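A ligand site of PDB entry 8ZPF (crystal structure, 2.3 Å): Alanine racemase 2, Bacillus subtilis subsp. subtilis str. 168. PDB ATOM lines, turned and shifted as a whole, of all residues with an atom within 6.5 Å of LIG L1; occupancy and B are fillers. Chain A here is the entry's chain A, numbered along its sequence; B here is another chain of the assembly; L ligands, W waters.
An oxygen (O1) of LG2 L2 is in hydrogen-bond range of an oxygen (O1) of LIG L1 (3.1 Å).
Water W2 lies within hydrogen-bond range of an oxygen (O1) of LIG L1 and the guanidinium group of Arg 143.
Water W1 lies within hydrogen-bond range of an oxygen (O3) of LIG L1 (2.7 Å), the backbone NH of Ala 215 (3.1 Å) and the side-chain amide nitrogen of Asn 213 (3.4 Å).
Merely in contact with LIG L1: Lys 43 (3.1 Å), His 173 (3.1 Å), Arg 143 (3.7 Å), Tyr 276 of chain B (3.9 Å), Asn 213 (3.96 Å) and Leu 89 (3.97 Å).
The nearest printed residue that does not touch LIG L1 is Val 41 (4.01 Å).
O5 of LIG L1 sits at hydrogen-bond distance from N of Thr 214 (3.2 Å).
The side-chain hydroxyl (OG1) of Thr 214 is in hydrogen-bond range of an oxygen (O5) of LIG L1 (2.6 Å).
OH of Tyr 368 sits at hydrogen-bond distance from O3 of LIG L1, 2.7 Å away.
An oxygen (O4) of LIG L1 is in hydrogen-bond range of the backbone NH (N) of Ile 232 (2.8 Å).
NE of Arg 229 sits at hydrogen-bond distance from N1 of LIG L1.
An oxygen (O4) of LIG L1 lies within hydrogen-bond range of the side-chain hydroxyl (OH) of Tyr 47, at 3.0 Å.
An oxygen (O5) of LIG L1 is in hydrogen-bond range of the backbone NH (N) of Gly 231 (3.4 Å).
O1 of LG2 L2 is in salt-bridge range of NZ of Lys 43.
The guanidinium group (NH1) of Arg 143 lies within salt-bridge range of an oxygen (O2) of LG2 L2, at 3.5 Å.
O1 of LG2 L2 is in hydrogen-bond range of OH of Tyr 276 of chain B (3.3 Å).
O2 of LG2 L2 sits at hydrogen-bond distance from N of Met 324 of chain B (2.8 Å).
The backbone NH (N) of Gly 231 sits at hydrogen-bond distance from the side-chain hydroxyl (OG1) of Thr 214, at 3.3 Å.
NH2 of Arg 229 sits at hydrogen-bond distance from ND1 of His 173.
O of Cys 212 sits at hydrogen-bond distance from N of Arg 229, 3.2 Å away.
NH2 of Arg 229 sits at hydrogen-bond distance from O of Thr 172 (3.1 Å).
NZ of Lys 43 lies within salt-bridge range of OD2 of Asp 325 of chain B, 3.5 Å away.
A ring nitrogen (NE2) of His 173 lies within hydrogen-bond range of the side-chain hydroxyl (OH) of Tyr 276 of chain B.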
ATOM      1  N   VAL A  41       7.229 -13.774  20.101  1.00  0.00           N
ATOM      2  CA  VAL A  41       8.286 -14.022  21.093  1.00  0.00           C
ATOM      3  C   VAL A  41       8.815 -15.460  20.953  1.00  0.00           C
ATOM      4  O   VAL A  41       8.077 -16.427  21.213  1.00  0.00           O
ATOM      5  CB  VAL A  41       7.788 -13.740  22.513  1.00  0.00           C
ATOM      6  CG1 VAL A  41       8.963 -13.785  23.525  1.00  0.00           C
ATOM      7  CG2 VAL A  41       7.082 -12.375  22.554  1.00  0.00           C
ATOM      8  N   LYS A  43      12.163 -16.562  22.178  1.00  0.00           N
ATOM      9  CA  LYS A  43      13.307 -16.766  23.063  1.00  0.00           C
ATOM     10  C   LYS A  43      13.281 -18.181  23.671  1.00  0.00           C
ATOM     11  O   LYS A  43      12.269 -18.896  23.627  1.00  0.00           O
ATOM     12  CB  LYS A  43      13.302 -15.709  24.162  1.00  0.00           C
ATOM     13  CG  LYS A  43      12.289 -15.991  25.241  1.00  0.00           C
ATOM     14  CD  LYS A  43      11.865 -14.750  26.025  1.00  0.00           C
ATOM     15  CE  LYS A  43      11.237 -15.191  27.348  1.00  0.00           C
ATOM     16  NZ  LYS A  43      10.648 -14.081  28.116  1.00  0.00           N
ATOM     17  N   TYR A  47      10.508 -21.431  23.139  1.00  0.00           N
ATOM     18  CA  TYR A  47       9.856 -22.074  24.291  1.00  0.00           C
ATOM     19  C   TYR A  47       9.984 -23.601  24.231  1.00  0.00           C
ATOM     20  O   TYR A  47       9.049 -24.348  24.594  1.00  0.00           O
ATOM     21  CB  TYR A  47       8.380 -21.661  24.418  1.00  0.00           C
ATOM     22  CG  TYR A  47       8.101 -20.231  24.897  1.00  0.00           C
ATOM     23  CD1 TYR A  47       9.007 -19.182  24.664  1.00  0.00           C
ATOM     24  CD2 TYR A  47       6.914 -19.937  25.568  1.00  0.00           C
ATOM     25  CE1 TYR A  47       8.722 -17.864  25.095  1.00  0.00           C
ATOM     26  CE2 TYR A  47       6.617 -18.619  26.012  1.00  0.00           C
ATOM     27  CZ  TYR A  47       7.513 -17.603  25.776  1.00  0.00           C
ATOM     28  OH  TYR A  47       7.185 -16.329  26.214  1.00  0.00           O
ATOM     29  N   LEU A  89      15.189  -8.443  24.935  1.00  0.00           N
ATOM     30  CA  LEU A  89      14.336  -8.078  26.059  1.00  0.00           C
ATOM     31  C   LEU A  89      15.066  -7.953  27.385  1.00  0.00           C
ATOM     32  O   LEU A  89      14.582  -7.259  28.292  1.00  0.00           O
ATOM     33  CB  LEU A  89      13.218  -9.111  26.203  1.00  0.00           C
ATOM     34  CG  LEU A  89      12.005  -8.933  25.284  1.00  0.00           C
ATOM     35  CD1 LEU A  89      10.944  -9.998  25.601  1.00  0.00           C
ATOM     36  CD2 LEU A  89      11.433  -7.521  25.406  1.00  0.00           C
ATOM     37  N   ARG A 143      11.800  -5.459  37.728  1.00  0.00           N
ATOM     38  CA  ARG A 143      12.905  -6.242  37.194  1.00  0.00           C
ATOM     39  C   ARG A 143      13.939  -5.305  36.546  1.00  0.00           C
ATOM     40  O   ARG A 143      15.016  -5.101  37.119  1.00  0.00           O
ATOM     41  CB  ARG A 143      12.372  -7.273  36.196  1.00  0.00           C
ATOM     42  CG  ARG A 143      13.407  -8.238  35.537  1.00  0.00           C
ATOM     43  CD  ARG A 143      12.695  -9.453  34.868  1.00  0.00           C
ATOM     44  NE  ARG A 143      11.677  -9.064  33.892  1.00  0.00           N
ATOM     45  CZ  ARG A 143      10.905  -9.891  33.206  1.00  0.00           C
ATOM     46  NH1 ARG A 143      10.984 -11.202  33.359  1.00  0.00           N
ATOM     47  NH2 ARG A 143      10.004  -9.392  32.351  1.00  0.00           N
ATOM     48  N   PHE A 171       8.187   0.754  26.028  1.00  0.00           N
ATOM     49  CA  PHE A 171       7.278  -0.293  26.490  1.00  0.00           C
ATOM     50  C   PHE A 171       7.305  -0.436  28.018  1.00  0.00           C
ATOM     51  O   PHE A 171       8.145   0.158  28.709  1.00  0.00           O
ATOM     52  CB  PHE A 171       7.589  -1.652  25.834  1.00  0.00           C
ATOM     53  CG  PHE A 171       8.945  -2.244  26.212  1.00  0.00           C
ATOM     54  CD1 PHE A 171      10.116  -1.861  25.539  1.00  0.00           C
ATOM     55  CD2 PHE A 171       9.041  -3.239  27.167  1.00  0.00           C
ATOM     56  CE1 PHE A 171      11.341  -2.446  25.856  1.00  0.00           C
ATOM     57  CE2 PHE A 171      10.264  -3.826  27.474  1.00  0.00           C
ATOM     58  CZ  PHE A 171      11.422  -3.428  26.822  1.00  0.00           C
ATOM     59  N   THR A 172       6.381  -1.261  28.510  1.00  0.00           N
ATOM     60  CA  THR A 172       6.282  -1.648  29.914  1.00  0.00           C
ATOM     61  C   THR A 172       5.837  -3.113  29.995  1.00  0.00           C
ATOM     62  O   THR A 172       5.607  -3.758  28.968  1.00  0.00           O
ATOM     63  CB  THR A 172       5.331  -0.706  30.677  1.00  0.00           C
ATOM     64  OG1 THR A 172       5.554  -0.824  32.082  1.00  0.00           O
ATOM     65  CG2 THR A 172       3.828  -1.008  30.334  1.00  0.00           C
ATOM     66  N   HIS A 173       5.715  -3.645  31.216  1.00  0.00           N
ATOM     67  CA  HIS A 173       5.310  -5.040  31.401  1.00  0.00           C
ATOM     68  C   HIS A 173       4.389  -5.214  32.617  1.00  0.00           C
ATOM     69  O   HIS A 173       4.692  -4.712  33.703  1.00  0.00           O
ATOM     70  CB  HIS A 173       6.553  -5.956  31.513  1.00  0.00           C
ATOM     71  CG  HIS A 173       6.244  -7.400  31.255  1.00  0.00           C
ATOM     72  ND1 HIS A 173       5.809  -7.858  30.028  1.00  0.00           N
ATOM     73  CD2 HIS A 173       6.288  -8.481  32.071  1.00  0.00           C
ATOM     74  CE1 HIS A 173       5.585  -9.163  30.099  1.00  0.00           C
ATOM     75  NE2 HIS A 173       5.882  -9.567  31.322  1.00  0.00           N
ATOM     76  N   CYS A 212       1.261  -4.996  25.968  1.00  0.00           N
ATOM     77  CA  CYS A 212       0.480  -6.200  26.253  1.00  0.00           C
ATOM     78  C   CYS A 212       1.285  -7.484  26.053  1.00  0.00           C
ATOM     79  O   CYS A 212       2.185  -7.550  25.211  1.00  0.00           O
ATOM     80  CB  CYS A 212      -0.750  -6.274  25.338  1.00  0.00           C
ATOM     81  SG  CYS A 212      -2.153  -5.194  25.770  1.00  0.00           S
ATOM     82  N   ASN A 213       0.922  -8.531  26.812  1.00  0.00           N
ATOM     83  CA  ASN A 213       1.349  -9.921  26.608  1.00  0.00           C
ATOM     84  C   ASN A 213       0.105 -10.778  26.261  1.00  0.00           C
ATOM     85  O   ASN A 213      -1.000 -10.238  26.099  1.00  0.00           O
ATOM     86  CB  ASN A 213       2.122 -10.465  27.826  1.00  0.00           C
ATOM     87  CG  ASN A 213       1.305 -10.390  29.139  1.00  0.00           C
ATOM     88  OD1 ASN A 213       0.144  -9.956  29.143  1.00  0.00           O
ATOM     89  ND2 ASN A 213       1.919 -10.807  30.255  1.00  0.00           N
ATOM     90  N   THR A 214       0.288 -12.101  26.139  1.00  0.00           N
ATOM     91  CA  THR A 214      -0.810 -12.972  25.707  1.00  0.00           C
ATOM     92  C   THR A 214      -2.074 -12.745  26.550  1.00  0.00           C
ATOM     93  O   THR A 214      -3.172 -12.561  26.004  1.00  0.00           O
ATOM     94  CB  THR A 214      -0.403 -14.455  25.754  1.00  0.00           C
ATOM     95  OG1 THR A 214       0.740 -14.680  24.933  1.00  0.00           O
ATOM     96  CG2 THR A 214      -1.554 -15.363  25.256  1.00  0.00           C
ATOM     97  N   ALA A 215      -1.937 -12.790  27.882  1.00  0.00           N
ATOM     98  CA  ALA A 215      -3.086 -12.576  28.770  1.00  0.00           C
ATOM     99  C   ALA A 215      -3.612 -11.157  28.664  1.00  0.00           C
ATOM    100  O   ALA A 215      -4.824 -10.934  28.648  1.00  0.00           O
ATOM    101  CB  ALA A 215      -2.697 -12.894  30.217  1.00  0.00           C
ATOM    102  N   ARG A 229       2.986  -8.243  22.143  1.00  0.00           N
ATOM    103  CA  ARG A 229       4.020  -9.297  22.165  1.00  0.00           C
ATOM    104  C   ARG A 229       3.349 -10.627  22.529  1.00  0.00           C
ATOM    105  O   ARG A 229       3.029 -10.881  23.686  1.00  0.00           O
ATOM    106  CB  ARG A 229       5.153  -8.927  23.130  1.00  0.00           C
ATOM    107  CG  ARG A 229       5.672  -7.492  22.958  1.00  0.00           C
ATOM    108  CD  ARG A 229       6.789  -7.060  23.965  1.00  0.00           C
ATOM    109  NE  ARG A 229       6.409  -7.203  25.369  1.00  0.00           N
ATOM    110  CZ  ARG A 229       5.902  -6.237  26.141  1.00  0.00           C
ATOM    111  NH1 ARG A 229       5.627  -5.034  25.672  1.00  0.00           N
ATOM    112  NH2 ARG A 229       5.677  -6.501  27.428  1.00  0.00           N
ATOM    113  N   LEU A 230       3.157 -11.482  21.517  1.00  0.00           N
ATOM    114  CA  LEU A 230       2.446 -12.752  21.637  1.00  0.00           C
ATOM    115  C   LEU A 230       3.453 -13.889  21.847  1.00  0.00           C
ATOM    116  O   LEU A 230       4.241 -14.200  20.941  1.00  0.00           O
ATOM    117  CB  LEU A 230       1.607 -12.982  20.373  1.00  0.00           C
ATOM    118  CG  LEU A 230       0.858 -14.288  20.114  1.00  0.00           C
ATOM    119  CD1 LEU A 230      -0.513 -14.293  20.754  1.00  0.00           C
ATOM    120  CD2 LEU A 230       0.723 -14.512  18.619  1.00  0.00           C
ATOM    121  N   GLY A 231       3.434 -14.517  23.028  1.00  0.00           N
ATOM    122  CA  GLY A 231       4.350 -15.599  23.367  1.00  0.00           C
ATOM    123  C   GLY A 231       3.704 -16.971  23.539  1.00  0.00           C
ATOM    124  O   GLY A 231       3.566 -17.716  22.556  1.00  0.00           O
ATOM    125  N   ILE A 232       3.288 -17.314  24.762  1.00  0.00           N
ATOM    126  CA  ILE A 232       2.760 -18.647  25.070  1.00  0.00           C
ATOM    127  C   ILE A 232       1.552 -19.006  24.210  1.00  0.00           C
ATOM    128  O   ILE A 232       1.342 -20.184  23.900  1.00  0.00           O
ATOM    129  CB  ILE A 232       2.427 -18.762  26.584  1.00  0.00           C
ATOM    130  CG1 ILE A 232       2.086 -20.199  27.004  1.00  0.00           C
ATOM    131  CG2 ILE A 232       1.274 -17.812  26.988  1.00  0.00           C
ATOM    132  CD1 ILE A 232       3.311 -21.112  27.202  1.00  0.00           C
ATOM    133  N   GLY A 233       0.732 -18.013  23.840  1.00  0.00           N
ATOM    134  CA  GLY A 233      -0.416 -18.287  22.982  1.00  0.00           C
ATOM    135  C   GLY A 233      -0.040 -18.728  21.586  1.00  0.00           C
ATOM    136  O   GLY A 233      -0.833 -19.411  20.915  1.00  0.00           O
ATOM    137  N   PRO A 239      -2.248 -18.783  29.333  1.00  0.00           N
ATOM    138  CA  PRO A 239      -1.431 -18.261  30.447  1.00  0.00           C
ATOM    139  C   PRO A 239      -1.835 -18.787  31.820  1.00  0.00           C
ATOM    140  O   PRO A 239      -0.963 -19.064  32.644  1.00  0.00           O
ATOM    141  CB  PRO A 239      -1.627 -16.737  30.353  1.00  0.00           C
ATOM    142  CG  PRO A 239      -2.434 -16.482  29.066  1.00  0.00           C
ATOM    143  CD  PRO A 239      -2.585 -17.764  28.332  1.00  0.00           C
ATOM    144  N   TYR A 368       4.659 -23.304  31.021  1.00  0.00           N
ATOM    145  CA  TYR A 368       5.897 -22.627  30.618  1.00  0.00           C
ATOM    146  C   TYR A 368       7.169 -23.458  30.894  1.00  0.00           C
ATOM    147  O   TYR A 368       8.074 -23.501  30.057  1.00  0.00           O
ATOM    148  CB  TYR A 368       6.047 -21.294  31.353  1.00  0.00           C
ATOM    149  CG  TYR A 368       5.111 -20.152  30.963  1.00  0.00           C
ATOM    150  CD1 TYR A 368       3.831 -20.106  31.452  1.00  0.00           C
ATOM    151  CD2 TYR A 368       5.546 -19.101  30.139  1.00  0.00           C
ATOM    152  CE1 TYR A 368       2.959 -19.048  31.130  1.00  0.00           C
ATOM    153  CE2 TYR A 368       4.692 -18.036  29.802  1.00  0.00           C
ATOM    154  CZ  TYR A 368       3.392 -18.019  30.311  1.00  0.00           C
ATOM    155  OH  TYR A 368       2.518 -16.966  30.011  1.00  0.00           O
ATOM    156  N   TYR B 276       6.331 -11.687  39.019  1.00  0.00           N
ATOM    157  CA  TYR B 276       4.974 -12.130  38.701  1.00  0.00           C
ATOM    158  C   TYR B 276       4.240 -12.581  39.962  1.00  0.00           C
ATOM    159  O   TYR B 276       4.837 -13.152  40.885  1.00  0.00           O
ATOM    160  CB  TYR B 276       4.945 -13.294  37.703  1.00  0.00           C
ATOM    161  CG  TYR B 276       5.487 -13.006  36.312  1.00  0.00           C
ATOM    162  CD1 TYR B 276       4.871 -12.098  35.457  1.00  0.00           C
ATOM    163  CD2 TYR B 276       6.612 -13.695  35.839  1.00  0.00           C
ATOM    164  CE1 TYR B 276       5.391 -11.848  34.172  1.00  0.00           C
ATOM    165  CE2 TYR B 276       7.132 -13.464  34.568  1.00  0.00           C
ATOM    166  CZ  TYR B 276       6.527 -12.541  33.749  1.00  0.00           C
ATOM    167  OH  TYR B 276       7.072 -12.345  32.502  1.00  0.00           O
ATOM    168  N   MET B 324      11.660 -16.914  33.372  1.00  0.00           N
ATOM    169  CA  MET B 324      12.274 -17.784  32.353  1.00  0.00           C
ATOM    170  C   MET B 324      13.759 -17.464  32.146  1.00  0.00           C
ATOM    171  O   MET B 324      14.571 -18.388  31.943  1.00  0.00           O
ATOM    172  CB  MET B 324      11.489 -17.674  31.051  1.00  0.00           C
ATOM    173  CG  MET B 324      12.011 -18.493  29.882  1.00  0.00           C
ATOM    174  SD  MET B 324      10.856 -18.628  28.479  1.00  0.00           S
ATOM    175  CE  MET B 324       9.376 -19.251  29.267  1.00  0.00           C
ATOM    176  N   ASP B 325      14.136 -16.173  32.195  1.00  0.00           N
ATOM    177  CA  ASP B 325      15.475 -15.689  31.876  1.00  0.00           C
ATOM    178  C   ASP B 325      16.187 -14.970  33.020  1.00  0.00           C
ATOM    179  O   ASP B 325      17.382 -14.683  32.871  1.00  0.00           O
ATOM    180  CB  ASP B 325      15.448 -14.706  30.682  1.00  0.00           C
ATOM    181  CG  ASP B 325      14.764 -15.275  29.440  1.00  0.00           C
ATOM    182  OD1 ASP B 325      14.915 -16.498  29.168  1.00  0.00           O
ATOM    183  OD2 ASP B 325      14.058 -14.504  28.743  1.00  0.00           O
ATOM    184  N   MET B 326      15.501 -14.663  34.127  1.00  0.00           N
ATOM    185  CA  MET B 326      16.073 -13.788  35.150  1.00  0.00           C
ATOM    186  C   MET B 326      15.532 -14.143  36.533  1.00  0.00           C
ATOM    187  O   MET B 326      14.428 -14.701  36.659  1.00  0.00           O
ATOM    188  CB  MET B 326      15.776 -12.311  34.856  1.00  0.00           C
ATOM    189  CG  MET B 326      16.326 -11.805  33.533  1.00  0.00           C
ATOM    190  SD  MET B 326      16.016 -10.035  33.305  1.00  0.00           S
ATOM    191  CE  MET B 326      14.718 -10.068  32.062  1.00  0.00           C
HETATM  192  N1  LIG L   1       6.711  -9.624  26.852  1.00  0.00           N
HETATM  193  C1  LIG L   1       7.654  -9.754  27.809  1.00  0.00           C
HETATM  194  C2  LIG L   1       8.381  -8.513  28.397  1.00  0.00           C
HETATM  195  C3  LIG L   1       7.989 -11.013  28.309  1.00  0.00           C
HETATM  196  O1  LIG L   1       8.976 -11.169  29.316  1.00  0.00           O
HETATM  197  C4  LIG L   1       7.328 -12.109  27.763  1.00  0.00           C
HETATM  198  C5  LIG L   1       7.652 -13.522  28.267  1.00  0.00           C
HETATM  199  C6  LIG L   1       6.364 -11.918  26.756  1.00  0.00           C
HETATM  200  C7  LIG L   1       6.057 -10.641  26.329  1.00  0.00           C
HETATM  201  C8  LIG L   1       5.638 -13.143  26.216  1.00  0.00           C
HETATM  202  O2  LIG L   1       5.050 -13.591  27.409  1.00  0.00           O
HETATM  203  P1  LIG L   1       3.748 -14.565  27.387  1.00  0.00           P
HETATM  204  O3  LIG L   1       3.076 -14.618  28.763  1.00  0.00           O
HETATM  205  O4  LIG L   1       4.286 -15.944  27.027  1.00  0.00           O
HETATM  206  O5  LIG L   1       2.799 -14.072  26.336  1.00  0.00           O
HETATM  207  N1  LG2 L   2       8.258 -16.181  33.052  1.00  0.00           N
HETATM  208  C1  LG2 L   2       8.559 -15.802  31.665  1.00  0.00           C
HETATM  209  C2  LG2 L   2       9.515 -14.660  31.704  1.00  0.00           C
HETATM  210  O1  LG2 L   2       9.553 -13.792  30.833  1.00  0.00           O
HETATM  211  C3  LG2 L   2       7.294 -15.408  30.877  1.00  0.00           C
HETATM  212  O2  LG2 L   2      10.294 -14.606  32.652  1.00  0.00           O
HETATM  213  O   HOH W   1       0.595 -13.798  29.369  1.00  0.00           O
HETATM  214  O   HOH W   2      11.309 -10.539  29.411  1.00  0.00           O
